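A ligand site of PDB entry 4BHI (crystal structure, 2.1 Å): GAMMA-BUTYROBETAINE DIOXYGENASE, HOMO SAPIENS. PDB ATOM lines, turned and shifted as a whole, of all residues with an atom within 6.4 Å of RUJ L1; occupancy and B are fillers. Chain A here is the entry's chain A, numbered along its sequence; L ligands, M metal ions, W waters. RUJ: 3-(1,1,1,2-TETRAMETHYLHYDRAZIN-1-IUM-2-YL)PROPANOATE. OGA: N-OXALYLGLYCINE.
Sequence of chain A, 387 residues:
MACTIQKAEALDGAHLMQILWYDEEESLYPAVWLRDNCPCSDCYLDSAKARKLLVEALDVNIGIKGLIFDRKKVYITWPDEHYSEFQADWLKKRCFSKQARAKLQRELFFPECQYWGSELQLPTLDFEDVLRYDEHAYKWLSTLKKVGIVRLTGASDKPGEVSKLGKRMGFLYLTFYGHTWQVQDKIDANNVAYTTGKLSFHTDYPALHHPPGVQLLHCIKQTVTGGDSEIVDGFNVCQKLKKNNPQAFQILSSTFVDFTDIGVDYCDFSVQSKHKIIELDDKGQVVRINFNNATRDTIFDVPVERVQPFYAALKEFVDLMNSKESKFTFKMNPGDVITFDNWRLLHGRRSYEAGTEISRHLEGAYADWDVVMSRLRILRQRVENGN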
ATOM      1  N   THR A 175     -23.112  12.635  -7.079  1.00  0.00           N
ATOM      2  CA  THR A 175     -22.975  11.283  -7.626  1.00  0.00           C
ATOM      3  C   THR A 175     -24.154  10.418  -7.165  1.00  0.00           C
ATOM      4  O   THR A 175     -25.037  10.880  -6.444  1.00  0.00           O
ATOM      5  CB  THR A 175     -21.647  10.616  -7.206  1.00  0.00           C
ATOM      6  OG1 THR A 175     -21.699  10.225  -5.819  1.00  0.00           O
ATOM      7  CG2 THR A 175     -20.473  11.564  -7.388  1.00  0.00           C
ATOM      8  N   TYR A 177     -24.139   8.239  -5.057  1.00  0.00           N
ATOM      9  CA  TYR A 177     -24.122   8.090  -3.596  1.00  0.00           C
ATOM     10  C   TYR A 177     -24.646   9.348  -2.861  1.00  0.00           C
ATOM     11  O   TYR A 177     -24.749   9.331  -1.645  1.00  0.00           O
ATOM     12  CB  TYR A 177     -22.747   7.660  -3.094  1.00  0.00           C
ATOM     13  CG  TYR A 177     -22.441   6.234  -3.517  1.00  0.00           C
ATOM     14  CD1 TYR A 177     -22.966   5.152  -2.799  1.00  0.00           C
ATOM     15  CD2 TYR A 177     -21.702   5.968  -4.664  1.00  0.00           C
ATOM     16  CE1 TYR A 177     -22.729   3.844  -3.195  1.00  0.00           C
ATOM     17  CE2 TYR A 177     -21.460   4.653  -5.081  1.00  0.00           C
ATOM     18  CZ  TYR A 177     -21.964   3.595  -4.314  1.00  0.00           C
ATOM     19  OH  TYR A 177     -21.743   2.295  -4.697  1.00  0.00           O
ATOM     20  N   TRP A 181     -22.574  11.718   1.685  1.00  0.00           N
ATOM     21  CA  TRP A 181     -22.839  10.312   1.977  1.00  0.00           C
ATOM     22  C   TRP A 181     -22.216   9.972   3.323  1.00  0.00           C
ATOM     23  O   TRP A 181     -21.252  10.617   3.758  1.00  0.00           O
ATOM     24  CB  TRP A 181     -22.290   9.375   0.864  1.00  0.00           C
ATOM     25  CG  TRP A 181     -21.111   9.923   0.109  1.00  0.00           C
ATOM     26  CD1 TRP A 181     -21.164  10.632  -1.044  1.00  0.00           C
ATOM     27  CD2 TRP A 181     -19.733   9.810   0.451  1.00  0.00           C
ATOM     28  NE1 TRP A 181     -19.906  10.999  -1.440  1.00  0.00           N
ATOM     29  CE2 TRP A 181     -19.010  10.512  -0.536  1.00  0.00           C
ATOM     30  CE3 TRP A 181     -19.042   9.198   1.482  1.00  0.00           C
ATOM     31  CZ2 TRP A 181     -17.628  10.597  -0.522  1.00  0.00           C
ATOM     32  CZ3 TRP A 181     -17.671   9.302   1.501  1.00  0.00           C
ATOM     33  CH2 TRP A 181     -16.978   9.977   0.493  1.00  0.00           C
ATOM     34  N   VAL A 183     -20.401   7.330   5.723  1.00  0.00           N
ATOM     35  CA  VAL A 183     -19.561   6.152   5.805  1.00  0.00           C
ATOM     36  C   VAL A 183     -19.780   5.532   7.168  1.00  0.00           C
ATOM     37  O   VAL A 183     -19.309   6.043   8.180  1.00  0.00           O
ATOM     38  CB  VAL A 183     -18.069   6.471   5.590  1.00  0.00           C
ATOM     39  CG1 VAL A 183     -17.240   5.211   5.640  1.00  0.00           C
ATOM     40  CG2 VAL A 183     -17.878   7.159   4.264  1.00  0.00           C
ATOM     41  N   ASN A 190     -24.595  -1.474   0.056  1.00  0.00           N
ATOM     42  CA  ASN A 190     -24.404  -1.366  -1.381  1.00  0.00           C
ATOM     43  C   ASN A 190     -22.933  -1.089  -1.778  1.00  0.00           C
ATOM     44  O   ASN A 190     -22.633  -0.931  -2.959  1.00  0.00           O
ATOM     45  CB  ASN A 190     -25.357  -0.325  -1.984  1.00  0.00           C
ATOM     46  CG  ASN A 190     -25.064   1.104  -1.538  1.00  0.00           C
ATOM     47  OD1 ASN A 190     -24.024   1.394  -0.968  1.00  0.00           O
ATOM     48  ND2 ASN A 190     -25.982   2.000  -1.841  1.00  0.00           N
ATOM     49  N   ASN A 191     -22.022  -1.080  -0.808  1.00  0.00           N
ATOM     50  CA  ASN A 191     -20.634  -0.701  -1.065  1.00  0.00           C
ATOM     51  C   ASN A 191     -19.779  -1.200   0.086  1.00  0.00           C
ATOM     52  O   ASN A 191     -20.171  -1.076   1.255  1.00  0.00           O
ATOM     53  CB  ASN A 191     -20.519   0.843  -1.214  1.00  0.00           C
ATOM     54  CG  ASN A 191     -19.218   1.279  -1.895  1.00  0.00           C
ATOM     55  OD1 ASN A 191     -18.164   1.344  -1.262  1.00  0.00           O
ATOM     56  ND2 ASN A 191     -19.299   1.618  -3.170  1.00  0.00           N
ATOM     57  N   VAL A 192     -18.600  -1.739  -0.222  1.00  0.00           N
ATOM     58  CA  VAL A 192     -17.718  -2.222   0.837  1.00  0.00           C
ATOM     59  C   VAL A 192     -17.347  -1.077   1.804  1.00  0.00           C
ATOM     60  O   VAL A 192     -17.015  -1.330   2.957  1.00  0.00           O
ATOM     61  CB  VAL A 192     -16.411  -2.860   0.291  1.00  0.00           C
ATOM     62  CG1 VAL A 192     -16.717  -4.060  -0.600  1.00  0.00           C
ATOM     63  CG2 VAL A 192     -15.587  -1.837  -0.454  1.00  0.00           C
ATOM     64  N   ALA A 193     -17.376   0.162   1.326  1.00  0.00           N
ATOM     65  CA  ALA A 193     -17.146   1.311   2.223  1.00  0.00           C
ATOM     66  C   ALA A 193     -18.091   1.292   3.442  1.00  0.00           C
ATOM     67  O   ALA A 193     -17.700   1.658   4.550  1.00  0.00           O
ATOM     68  CB  ALA A 193     -17.271   2.621   1.468  1.00  0.00           C
ATOM     69  N   TYR A 194     -19.328   0.817   3.228  1.00  0.00           N
ATOM     70  CA  TYR A 194     -20.393   0.829   4.242  1.00  0.00           C
ATOM     71  C   TYR A 194     -20.455  -0.478   5.067  1.00  0.00           C
ATOM     72  O   TYR A 194     -21.551  -1.023   5.337  1.00  0.00           O
ATOM     73  CB  TYR A 194     -21.749   1.109   3.565  1.00  0.00           C
ATOM     74  CG  TYR A 194     -21.795   2.420   2.763  1.00  0.00           C
ATOM     75  CD1 TYR A 194     -20.979   3.504   3.106  1.00  0.00           C
ATOM     76  CD2 TYR A 194     -22.641   2.562   1.667  1.00  0.00           C
ATOM     77  CE1 TYR A 194     -20.997   4.666   2.391  1.00  0.00           C
ATOM     78  CE2 TYR A 194     -22.659   3.746   0.930  1.00  0.00           C
ATOM     79  CZ  TYR A 194     -21.842   4.786   1.317  1.00  0.00           C
ATOM     80  OH  TYR A 194     -21.819   5.976   0.660  1.00  0.00           O
ATOM     81  N   HIS A 202      -6.975   2.693  -2.339  1.00  0.00           N
ATOM     82  CA  HIS A 202      -7.741   2.897  -3.541  1.00  0.00           C
ATOM     83  C   HIS A 202      -7.971   4.382  -3.771  1.00  0.00           C
ATOM     84  O   HIS A 202      -7.743   5.195  -2.877  1.00  0.00           O
ATOM     85  CB  HIS A 202      -9.106   2.239  -3.361  1.00  0.00           C
ATOM     86  CG  HIS A 202      -9.927   2.868  -2.300  1.00  0.00           C
ATOM     87  ND1 HIS A 202      -9.744   2.592  -0.967  1.00  0.00           N
ATOM     88  CD2 HIS A 202     -10.888   3.815  -2.359  1.00  0.00           C
ATOM     89  CE1 HIS A 202     -10.581   3.333  -0.252  1.00  0.00           C
ATOM     90  NE2 HIS A 202     -11.303   4.057  -1.077  1.00  0.00           N
ATOM     91  N   THR A 203      -8.426   4.708  -4.975  1.00  0.00           N
ATOM     92  CA  THR A 203      -9.043   5.982  -5.280  1.00  0.00           C
ATOM     93  C   THR A 203     -10.540   5.737  -5.325  1.00  0.00           C
ATOM     94  O   THR A 203     -10.971   4.626  -5.615  1.00  0.00           O
ATOM     95  CB  THR A 203      -8.573   6.508  -6.650  1.00  0.00           C
ATOM     96  OG1 THR A 203      -8.863   5.544  -7.687  1.00  0.00           O
ATOM     97  CG2 THR A 203      -7.066   6.756  -6.633  1.00  0.00           C
ATOM     98  N   ASP A 204     -11.336   6.773  -5.042  1.00  0.00           N
ATOM     99  CA  ASP A 204     -12.797   6.685  -5.130  1.00  0.00           C
ATOM    100  C   ASP A 204     -13.289   6.859  -6.540  1.00  0.00           C
ATOM    101  O   ASP A 204     -12.822   7.702  -7.282  1.00  0.00           O
ATOM    102  CB  ASP A 204     -13.489   7.735  -4.256  1.00  0.00           C
ATOM    103  CG  ASP A 204     -13.683   7.289  -2.836  1.00  0.00           C
ATOM    104  OD1 ASP A 204     -12.850   6.498  -2.337  1.00  0.00           O
ATOM    105  OD2 ASP A 204     -14.677   7.744  -2.219  1.00  0.00           O
ATOM    106  N   TYR A 205     -14.241   5.992  -6.871  1.00  0.00           N
ATOM    107  CA  TYR A 205     -15.096   6.090  -8.050  1.00  0.00           C
ATOM    108  C   TYR A 205     -14.382   5.950  -9.383  1.00  0.00           C
ATOM    109  O   TYR A 205     -14.711   6.655 -10.326  1.00  0.00           O
ATOM    110  CB  TYR A 205     -15.918   7.354  -7.993  1.00  0.00           C
ATOM    111  CG  TYR A 205     -17.448   7.166  -7.915  1.00  0.00           C
ATOM    112  CD1 TYR A 205     -18.121   6.220  -8.706  1.00  0.00           C
ATOM    113  CD2 TYR A 205     -18.222   7.975  -7.109  1.00  0.00           C
ATOM    114  CE1 TYR A 205     -19.509   6.085  -8.674  1.00  0.00           C
ATOM    115  CE2 TYR A 205     -19.608   7.858  -7.079  1.00  0.00           C
ATOM    116  CZ  TYR A 205     -20.244   6.909  -7.861  1.00  0.00           C
ATOM    117  OH  TYR A 205     -21.621   6.814  -7.831  1.00  0.00           O
ATOM    118  N   PRO A 206     -13.439   4.997  -9.494  1.00  0.00           N
ATOM    119  CA  PRO A 206     -12.976   4.693 -10.870  1.00  0.00           C
ATOM    120  C   PRO A 206     -14.080   4.120 -11.775  1.00  0.00           C
ATOM    121  O   PRO A 206     -13.898   4.101 -12.986  1.00  0.00           O
ATOM    122  CB  PRO A 206     -11.888   3.644 -10.651  1.00  0.00           C
ATOM    123  CG  PRO A 206     -12.170   3.074  -9.328  1.00  0.00           C
ATOM    124  CD  PRO A 206     -12.745   4.179  -8.502  1.00  0.00           C
ATOM    125  N   ALA A 207     -15.227   3.698 -11.216  1.00  0.00           N
ATOM    126  CA  ALA A 207     -16.372   3.294 -12.054  1.00  0.00           C
ATOM    127  C   ALA A 207     -16.936   4.444 -12.888  1.00  0.00           C
ATOM    128  O   ALA A 207     -17.759   4.222 -13.766  1.00  0.00           O
ATOM    129  CB  ALA A 207     -17.486   2.710 -11.194  1.00  0.00           C
ATOM    130  N   GLN A 215     -11.739  14.928  -2.579  1.00  0.00           N
ATOM    131  CA  GLN A 215     -12.613  14.268  -1.628  1.00  0.00           C
ATOM    132  C   GLN A 215     -12.546  14.995  -0.304  1.00  0.00           C
ATOM    133  O   GLN A 215     -11.495  15.468   0.108  1.00  0.00           O
ATOM    134  CB  GLN A 215     -12.198  12.804  -1.435  1.00  0.00           C
ATOM    135  CG  GLN A 215     -13.183  11.998  -0.587  1.00  0.00           C
ATOM    136  CD  GLN A 215     -12.836  10.533  -0.446  1.00  0.00           C
ATOM    137  OE1 GLN A 215     -13.063   9.950   0.603  1.00  0.00           O
ATOM    138  NE2 GLN A 215     -12.300   9.919  -1.505  1.00  0.00           N
ATOM    139  N   ASP A 261     -20.160  -0.723 -11.037  1.00  0.00           N
ATOM    140  CA  ASP A 261     -20.903  -0.412  -9.800  1.00  0.00           C
ATOM    141  C   ASP A 261     -22.396  -0.461 -10.110  1.00  0.00           C
ATOM    142  O   ASP A 261     -22.906   0.315 -10.894  1.00  0.00           O
ATOM    143  CB  ASP A 261     -20.530   0.975  -9.222  1.00  0.00           C
ATOM    144  CG  ASP A 261     -20.890   1.118  -7.734  1.00  0.00           C
ATOM    145  OD1 ASP A 261     -21.071   0.101  -7.049  1.00  0.00           O
ATOM    146  OD2 ASP A 261     -20.994   2.273  -7.232  1.00  0.00           O
ATOM    147  N   ASN A 292      -9.721   1.103  -7.647  1.00  0.00           N
ATOM    148  CA  ASN A 292     -10.398   0.581  -6.476  1.00  0.00           C
ATOM    149  C   ASN A 292     -10.605  -0.921  -6.709  1.00  0.00           C
ATOM    150  O   ASN A 292     -11.156  -1.332  -7.729  1.00  0.00           O
ATOM    151  CB  ASN A 292     -11.712   1.314  -6.240  1.00  0.00           C
ATOM    152  CG  ASN A 292     -12.380   0.932  -4.914  1.00  0.00           C
ATOM    153  OD1 ASN A 292     -12.188  -0.169  -4.387  1.00  0.00           O
ATOM    154  ND2 ASN A 292     -13.173   1.841  -4.369  1.00  0.00           N
ATOM    155  N   ALA A 294     -12.214  -3.059  -4.985  1.00  0.00           N
ATOM    156  CA  ALA A 294     -13.569  -3.475  -4.718  1.00  0.00           C
ATOM    157  C   ALA A 294     -14.371  -3.428  -5.999  1.00  0.00           C
ATOM    158  O   ALA A 294     -15.145  -4.363  -6.298  1.00  0.00           O
ATOM    159  CB  ALA A 294     -14.205  -2.629  -3.611  1.00  0.00           C
ATOM    160  N   THR A 295     -14.169  -2.365  -6.777  1.00  0.00           N
ATOM    161  CA  THR A 295     -15.016  -2.082  -7.938  1.00  0.00           C
ATOM    162  C   THR A 295     -14.411  -2.471  -9.254  1.00  0.00           C
ATOM    163  O   THR A 295     -15.072  -2.372 -10.277  1.00  0.00           O
ATOM    164  CB  THR A 295     -15.476  -0.602  -8.006  1.00  0.00           C
ATOM    165  OG1 THR A 295     -14.366   0.278  -8.173  1.00  0.00           O
ATOM    166  CG2 THR A 295     -16.245  -0.246  -6.751  1.00  0.00           C
ATOM    167  N   HIS A 347      -6.091   6.063  -0.719  1.00  0.00           N
ATOM    168  CA  HIS A 347      -6.403   6.104   0.684  1.00  0.00           C
ATOM    169  C   HIS A 347      -7.020   4.806   1.090  1.00  0.00           C
ATOM    170  O   HIS A 347      -7.463   4.004   0.230  1.00  0.00           O
ATOM    171  CB  HIS A 347      -7.297   7.290   1.004  1.00  0.00           C
ATOM    172  CG  HIS A 347      -8.653   7.229   0.359  1.00  0.00           C
ATOM    173  ND1 HIS A 347      -8.833   7.440  -0.998  1.00  0.00           N
ATOM    174  CD2 HIS A 347      -9.867   6.945   0.866  1.00  0.00           C
ATOM    175  CE1 HIS A 347     -10.117   7.308  -1.289  1.00  0.00           C
ATOM    176  NE2 HIS A 347     -10.763   7.012  -0.171  1.00  0.00           N
ATOM    177  N   TYR A 366     -17.654  14.958  -2.662  1.00  0.00           N
ATOM    178  CA  TYR A 366     -16.689  15.141  -3.711  1.00  0.00           C
ATOM    179  C   TYR A 366     -16.760  16.553  -4.278  1.00  0.00           C
ATOM    180  O   TYR A 366     -17.803  17.201  -4.211  1.00  0.00           O
ATOM    181  CB  TYR A 366     -16.985  14.149  -4.832  1.00  0.00           C
ATOM    182  CG  TYR A 366     -16.886  12.690  -4.446  1.00  0.00           C
ATOM    183  CD1 TYR A 366     -15.711  12.165  -3.904  1.00  0.00           C
ATOM    184  CD2 TYR A 366     -17.962  11.836  -4.633  1.00  0.00           C
ATOM    185  CE1 TYR A 366     -15.611  10.826  -3.560  1.00  0.00           C
ATOM    186  CE2 TYR A 366     -17.879  10.486  -4.303  1.00  0.00           C
ATOM    187  CZ  TYR A 366     -16.692   9.981  -3.791  1.00  0.00           C
ATOM    188  OH  TYR A 366     -16.593   8.642  -3.446  1.00  0.00           O
HETATM  189  O4  RUJ L   1     -15.316   3.812  -5.464  1.00  0.00           O
HETATM  190  C5  RUJ L   1     -16.118   3.389  -4.615  1.00  0.00           C
HETATM  191  O7  RUJ L   1     -17.026   2.566  -4.918  1.00  0.00           O
HETATM  192  C6  RUJ L   1     -15.990   3.787  -3.143  1.00  0.00           C
HETATM  193  C3  RUJ L   1     -16.234   5.227  -2.776  1.00  0.00           C
HETATM  194  N2  RUJ L   1     -17.666   5.567  -2.736  1.00  0.00           N
HETATM  195  C21 RUJ L   1     -18.243   5.626  -4.066  1.00  0.00           C
HETATM  196  N1  RUJ L   1     -18.398   5.861  -1.597  1.00  0.00           N
HETATM  197  C8  RUJ L   1     -19.383   4.802  -1.302  1.00  0.00           C
HETATM  198  C9  RUJ L   1     -17.554   6.062  -0.398  1.00  0.00           C
HETATM  199  C10 RUJ L   1     -19.145   7.119  -1.778  1.00  0.00           C
HETATM  200  C1  OGA L   2     -14.480   5.148   1.421  1.00  0.00           C
HETATM  201  C2  OGA L   2     -13.297   5.386   2.262  1.00  0.00           C
HETATM  202  C4  OGA L   2     -12.467   5.818   4.468  1.00  0.00           C
HETATM  203  C5  OGA L   2     -12.844   5.412   5.864  1.00  0.00           C
HETATM  204  O1  OGA L   2     -14.325   4.916   0.192  1.00  0.00           O
HETATM  205  O2  OGA L   2     -15.614   5.185   1.991  1.00  0.00           O
HETATM  206  O2' OGA L   2     -12.156   5.417   1.780  1.00  0.00           O
HETATM  207  O3  OGA L   2     -12.017   5.746   6.693  1.00  0.00           O
HETATM  208  N1  OGA L   2     -13.541   5.571   3.546  1.00  0.00           N
HETATM  209  O4  OGA L   2     -13.905   4.804   6.124  1.00  0.00           O
HETATM  210 ZN    ZN M   1     -12.498   5.720  -0.368  1.00  0.00          ZN
HETATM  211  O   HOH W   1     -15.749   2.862  -8.343  1.00  0.00           O
HETATM  212  O   HOH W   2     -18.093   2.766  -7.231  1.00  0.00           O
HETATM  213  O   HOH W   3     -15.847   0.792  -2.964  1.00  0.00           O
HETATM  214  O   HOH W   4     -14.303   1.912  -1.100  1.00  0.00           O
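The side-chain amide nitrogen (ND2) of Asn 292 is in hydrogen-bond range of an oxygen (O4) of RUJ L1. ND2 of Asn 191 is in hydrogen-bond range of O7 of RUJ L1 (3.0 Å). A nitrogen (N2) of RUJ L1 lies close to the side-chain hydroxyl (OH) of Tyr 366 (3.3 Å). The backbone NH (N) of Tyr 205 lies within hydrogen-bond range of an oxygen (O4) of RUJ L1.
Water W2 bridges an oxygen (O7) of RUJ L1 (2.6 Å) and the side-chain carboxylate of Asp 261 (2.9 Å). Water W3 lies within hydrogen-bond range of O7 of RUJ L1 (2.9 Å), OD1 of Asn 191 (2.9 Å) and ND2 of Asn 292 (3.2 Å). Water W1 lies within hydrogen-bond range of OG1 of Thr 295, N of Ala 207 and O4 of RUJ L1.
The backbone NH (N) of Ala 193 sits at hydrogen-bond distance from the side-chain amide oxygen (OD1) of Asn 191, 3.0 Å away. ND2 of Asn 191 sits at hydrogen-bond distance from OH of Tyr 177 (3.0 Å). The side-chain amide nitrogen (NE2) of Gln 215 sits close to the side-chain carboxylate (OD2) of Asp 204 (3.3 Å). The side-chain carboxylate (OD2) of Asp 204 lies within hydrogen-bond range of the side-chain hydroxyl (OH) of Tyr 366 (2.4 Å). The side-chain carboxylate of Asp 261 lies within hydrogen-bond range of the side-chain hydroxyl of Tyr 177 (2.6 Å). OG1 of Thr 175 lies close to N of Tyr 177 (3.2 Å). OD1 of Asn 292 sits at hydrogen-bond distance from N of Ala 294 (3.0 Å).
Merely in contact with RUJ L1: Tyr 177, Trp 181, Ala 193, Tyr 194, Asp 204, Pro 206 and Thr 295. Hydrophobic or aromatic side chains within 4 Å of RUJ L1: Tyr 177, Trp 181, Ala 193, Tyr 194, Tyr 205 and Pro 206.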
